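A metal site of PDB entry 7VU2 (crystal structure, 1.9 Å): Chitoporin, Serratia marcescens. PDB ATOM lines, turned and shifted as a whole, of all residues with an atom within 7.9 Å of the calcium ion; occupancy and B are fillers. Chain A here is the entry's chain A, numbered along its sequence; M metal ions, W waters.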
ATOM      1  N   LYS A  23     -26.099  -4.574  26.872  1.00  0.00           N
ATOM      2  CA  LYS A  23     -25.231  -3.439  27.079  1.00  0.00           C
ATOM      3  C   LYS A  23     -25.045  -2.674  25.771  1.00  0.00           C
ATOM      4  O   LYS A  23     -24.732  -3.257  24.737  1.00  0.00           O
ATOM      5  CB  LYS A  23     -23.880  -3.902  27.625  1.00  0.00           C
ATOM      6  CG  LYS A  23     -22.941  -2.760  28.055  1.00  0.00           C
ATOM      7  CD  LYS A  23     -21.515  -3.279  28.258  1.00  0.00           C
ATOM      8  CE  LYS A  23     -21.349  -3.916  29.596  1.00  0.00           C
ATOM      9  NZ  LYS A  23     -19.915  -4.237  29.694  1.00  0.00           N
ATOM     10  N   LEU A  25     -22.939  -0.342  23.654  1.00  0.00           N
ATOM     11  CA  LEU A  25     -21.624   0.263  23.428  1.00  0.00           C
ATOM     12  C   LEU A  25     -21.550   1.019  22.093  1.00  0.00           C
ATOM     13  O   LEU A  25     -20.458   1.200  21.556  1.00  0.00           O
ATOM     14  CB  LEU A  25     -20.508  -0.780  23.478  1.00  0.00           C
ATOM     15  CG  LEU A  25     -20.365  -1.511  24.814  1.00  0.00           C
ATOM     16  CD1 LEU A  25     -19.106  -2.357  24.814  1.00  0.00           C
ATOM     17  CD2 LEU A  25     -20.351  -0.556  26.010  1.00  0.00           C
ATOM     18  N   TYR A  35     -27.299  -1.440  30.379  1.00  0.00           N
ATOM     19  CA  TYR A  35     -28.060  -2.576  29.860  1.00  0.00           C
ATOM     20  C   TYR A  35     -29.460  -2.075  29.545  1.00  0.00           C
ATOM     21  O   TYR A  35     -30.362  -2.107  30.386  1.00  0.00           O
ATOM     22  CB  TYR A  35     -28.079  -3.709  30.859  1.00  0.00           C
ATOM     23  CG  TYR A  35     -26.792  -4.482  30.994  1.00  0.00           C
ATOM     24  CD1 TYR A  35     -25.697  -3.953  31.673  1.00  0.00           C
ATOM     25  CD2 TYR A  35     -26.676  -5.760  30.458  1.00  0.00           C
ATOM     26  CE1 TYR A  35     -24.514  -4.689  31.822  1.00  0.00           C
ATOM     27  CE2 TYR A  35     -25.514  -6.514  30.597  1.00  0.00           C
ATOM     28  CZ  TYR A  35     -24.421  -5.964  31.271  1.00  0.00           C
ATOM     29  OH  TYR A  35     -23.271  -6.716  31.401  1.00  0.00           O
ATOM     30  N   LYS A 372     -13.060 -13.365  22.911  1.00  0.00           N
ATOM     31  CA  LYS A 372     -13.607 -14.376  23.799  1.00  0.00           C
ATOM     32  C   LYS A 372     -15.028 -13.976  24.204  1.00  0.00           C
ATOM     33  O   LYS A 372     -15.337 -12.796  24.351  1.00  0.00           O
ATOM     34  CB  LYS A 372     -12.762 -14.568  25.064  1.00  0.00           C
ATOM     35  CG  LYS A 372     -11.293 -14.890  24.829  1.00  0.00           C
ATOM     36  CD  LYS A 372     -10.630 -15.436  26.107  1.00  0.00           C
ATOM     37  CE  LYS A 372      -9.122 -15.653  25.920  1.00  0.00           C
ATOM     38  NZ  LYS A 372      -8.418 -14.342  25.771  1.00  0.00           N
ATOM     39  N   TYR A 401     -24.844 -13.287  29.616  1.00  0.00           N
ATOM     40  CA  TYR A 401     -23.916 -13.437  28.499  1.00  0.00           C
ATOM     41  C   TYR A 401     -22.878 -12.313  28.558  1.00  0.00           C
ATOM     42  O   TYR A 401     -23.228 -11.144  28.752  1.00  0.00           O
ATOM     43  CB  TYR A 401     -24.672 -13.448  27.158  1.00  0.00           C
ATOM     44  CG  TYR A 401     -23.741 -13.227  25.994  1.00  0.00           C
ATOM     45  CD1 TYR A 401     -22.929 -14.249  25.543  1.00  0.00           C
ATOM     46  CD2 TYR A 401     -23.649 -11.983  25.376  1.00  0.00           C
ATOM     47  CE1 TYR A 401     -22.047 -14.041  24.505  1.00  0.00           C
ATOM     48  CE2 TYR A 401     -22.786 -11.773  24.354  1.00  0.00           C
ATOM     49  CZ  TYR A 401     -21.986 -12.799  23.908  1.00  0.00           C
ATOM     50  OH  TYR A 401     -21.114 -12.565  22.867  1.00  0.00           O
ATOM     51  N   ASP A 402     -21.603 -12.684  28.374  1.00  0.00           N
ATOM     52  CA  ASP A 402     -20.493 -11.743  28.454  1.00  0.00           C
ATOM     53  C   ASP A 402     -19.640 -11.802  27.189  1.00  0.00           C
ATOM     54  O   ASP A 402     -18.970 -12.815  26.909  1.00  0.00           O
ATOM     55  CB  ASP A 402     -19.634 -12.015  29.701  1.00  0.00           C
ATOM     56  CG  ASP A 402     -18.680 -10.871  30.029  1.00  0.00           C
ATOM     57  OD1 ASP A 402     -18.628  -9.888  29.282  1.00  0.00           O
ATOM     58  OD2 ASP A 402     -17.957 -10.979  31.043  1.00  0.00           O
ATOM     59  N   ASN A 403     -19.669 -10.723  26.422  1.00  0.00           N
ATOM     60  CA  ASN A 403     -18.767 -10.462  25.301  1.00  0.00           C
ATOM     61  C   ASN A 403     -17.526  -9.802  25.881  1.00  0.00           C
ATOM     62  O   ASN A 403     -17.623  -8.740  26.473  1.00  0.00           O
ATOM     63  CB  ASN A 403     -19.477  -9.551  24.305  1.00  0.00           C
ATOM     64  CG  ASN A 403     -18.602  -9.116  23.129  1.00  0.00           C
ATOM     65  OD1 ASN A 403     -17.390  -8.921  23.227  1.00  0.00           O
ATOM     66  ND2 ASN A 403     -19.276  -8.880  21.993  1.00  0.00           N
ATOM     67  N   HIS A 404     -16.358 -10.427  25.727  1.00  0.00           N
ATOM     68  CA  HIS A 404     -15.159  -9.917  26.410  1.00  0.00           C
ATOM     69  C   HIS A 404     -14.402  -8.898  25.593  1.00  0.00           C
ATOM     70  O   HIS A 404     -13.165  -8.889  25.589  1.00  0.00           O
ATOM     71  CB  HIS A 404     -14.270 -11.079  26.808  1.00  0.00           C
ATOM     72  CG  HIS A 404     -14.886 -11.963  27.838  1.00  0.00           C
ATOM     73  ND1 HIS A 404     -14.952 -11.621  29.175  1.00  0.00           N
ATOM     74  CD2 HIS A 404     -15.507 -13.164  27.731  1.00  0.00           C
ATOM     75  CE1 HIS A 404     -15.563 -12.583  29.846  1.00  0.00           C
ATOM     76  NE2 HIS A 404     -15.906 -13.537  28.990  1.00  0.00           N
ATOM     77  N   THR A 405     -15.122  -8.034  24.892  1.00  0.00           N
ATOM     78  CA  THR A 405     -14.573  -6.931  24.131  1.00  0.00           C
ATOM     79  C   THR A 405     -15.464  -5.716  24.335  1.00  0.00           C
ATOM     80  O   THR A 405     -16.521  -5.796  24.966  1.00  0.00           O
ATOM     81  CB  THR A 405     -14.490  -7.216  22.624  1.00  0.00           C
ATOM     82  OG1 THR A 405     -15.811  -7.120  22.049  1.00  0.00           O
ATOM     83  CG2 THR A 405     -13.887  -8.577  22.353  1.00  0.00           C
ATOM     84  N   ASN A 406     -15.060  -4.588  23.753  1.00  0.00           N
ATOM     85  CA  ASN A 406     -15.901  -3.387  23.729  1.00  0.00           C
ATOM     86  C   ASN A 406     -16.510  -3.154  22.349  1.00  0.00           C
ATOM     87  O   ASN A 406     -16.963  -2.044  22.052  1.00  0.00           O
ATOM     88  CB  ASN A 406     -15.092  -2.167  24.160  1.00  0.00           C
ATOM     89  CG  ASN A 406     -14.570  -2.294  25.575  1.00  0.00           C
ATOM     90  OD1 ASN A 406     -15.165  -2.969  26.420  1.00  0.00           O
ATOM     91  ND2 ASN A 406     -13.454  -1.627  25.848  1.00  0.00           N
ATOM     92  N   PHE A 418     -23.034 -10.021  19.482  1.00  0.00           N
ATOM     93  CA  PHE A 418     -23.647  -8.882  20.133  1.00  0.00           C
ATOM     94  C   PHE A 418     -23.024  -8.696  21.516  1.00  0.00           C
ATOM     95  O   PHE A 418     -22.251  -9.551  21.995  1.00  0.00           O
ATOM     96  CB  PHE A 418     -25.172  -9.062  20.248  1.00  0.00           C
ATOM     97  CG  PHE A 418     -25.582 -10.417  20.735  1.00  0.00           C
ATOM     98  CD1 PHE A 418     -25.562 -10.712  22.090  1.00  0.00           C
ATOM     99  CD2 PHE A 418     -25.930 -11.415  19.848  1.00  0.00           C
ATOM    100  CE1 PHE A 418     -25.878 -11.979  22.549  1.00  0.00           C
ATOM    101  CE2 PHE A 418     -26.256 -12.695  20.291  1.00  0.00           C
ATOM    102  CZ  PHE A 418     -26.246 -12.964  21.643  1.00  0.00           C
ATOM    103  N   GLN A 419     -23.390  -7.610  22.177  1.00  0.00           N
ATOM    104  CA  GLN A 419     -22.758  -7.244  23.439  1.00  0.00           C
ATOM    105  C   GLN A 419     -23.441  -7.938  24.628  1.00  0.00           C
ATOM    106  O   GLN A 419     -24.431  -8.660  24.500  1.00  0.00           O
ATOM    107  CB  GLN A 419     -22.795  -5.725  23.602  1.00  0.00           C
ATOM    108  CG  GLN A 419     -21.492  -5.047  23.190  1.00  0.00           C
ATOM    109  CD  GLN A 419     -20.336  -5.499  24.042  1.00  0.00           C
ATOM    110  OE1 GLN A 419     -20.509  -5.776  25.228  1.00  0.00           O
ATOM    111  NE2 GLN A 419     -19.154  -5.595  23.446  1.00  0.00           N
ATOM    112  N   ASP A 420     -22.866  -7.686  25.828  1.00  0.00           N
ATOM    113  CA  ASP A 420     -23.276  -8.350  27.063  1.00  0.00           C
ATOM    114  C   ASP A 420     -24.787  -8.272  27.240  1.00  0.00           C
ATOM    115  O   ASP A 420     -25.417  -7.248  26.945  1.00  0.00           O
ATOM    116  CB  ASP A 420     -22.658  -7.672  28.286  1.00  0.00           C
ATOM    117  CG  ASP A 420     -21.141  -7.707  28.322  1.00  0.00           C
ATOM    118  OD1 ASP A 420     -20.506  -8.280  27.400  1.00  0.00           O
ATOM    119  OD2 ASP A 420     -20.579  -7.163  29.306  1.00  0.00           O
ATOM    120  N   GLU A 421     -25.360  -9.335  27.838  1.00  0.00           N
ATOM    121  CA  GLU A 421     -26.795  -9.403  28.016  1.00  0.00           C
ATOM    122  C   GLU A 421     -27.158 -10.053  29.341  1.00  0.00           C
ATOM    123  O   GLU A 421     -26.431 -10.881  29.870  1.00  0.00           O
ATOM    124  CB  GLU A 421     -27.481 -10.246  26.918  1.00  0.00           C
ATOM    125  CG  GLU A 421     -27.571  -9.605  25.555  1.00  0.00           C
ATOM    126  CD  GLU A 421     -28.318 -10.487  24.593  1.00  0.00           C
ATOM    127  OE1 GLU A 421     -28.530 -11.691  24.907  1.00  0.00           O
ATOM    128  OE2 GLU A 421     -28.722  -9.983  23.524  1.00  0.00           O
HETATM  129 CA    CA M   1     -18.229  -7.727  28.454  1.00  0.00          CA
HETATM  130  O   HOH W   1     -16.085  -8.700  29.475  1.00  0.00           O
HETATM  131  O   HOH W   2     -18.771  -5.688  27.230  1.00  0.00           O
HETATM  132  O   HOH W   3     -16.002  -6.812  28.177  1.00  0.00           O
HETATM  133  O   HOH W   4     -17.822  -6.363  30.514  1.00  0.00           O
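OG1 of Thr 405 is in hydrogen-bond range of OD1 of Asn 403, 2.7 Å away. The backbone carbonyl oxygen (O) of Phe 418 is in hydrogen-bond range of the side-chain amide nitrogen (ND2) of Asn 403, 3.0 Å away. The backbone NH (N) of Lys 23 lies within hydrogen-bond range of the backbone carbonyl oxygen (O) of Asp 420, 2.8 Å away. The side-chain carboxylate of Asp 420 lies close to the side-chain amide oxygen of Gln 419, 3.3 Å away. The side-chain carboxylate (OD2) of Asp 420 lies close to the side-chain hydroxyl (OH) of Tyr 35.
Three residues have an atom within 4 Å of the calcium ion: Asp 402, Asn 403 and Asp 420. The nearest printed residue that does not touch the calcium ion is Lys 23 (4.1 Å).
The calcium ion is bound by O of Asn 403, OD1 of Asp 402, water W3, water W2, water W4, OD2 of Asp 420, water W1 and OD1 of Asp 420.
Water W2 lies within hydrogen-bond range of OE1 of Gln 419 (2.7 Å), NZ of Lys 23 (3.1 Å) and O of Thr 405 (3.2 Å). Water W1 bridges a ring nitrogen (ND1) of His 404 (3.1 Å) and the side-chain carboxylate (OD2) of Asp 402 (3.3 Å).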
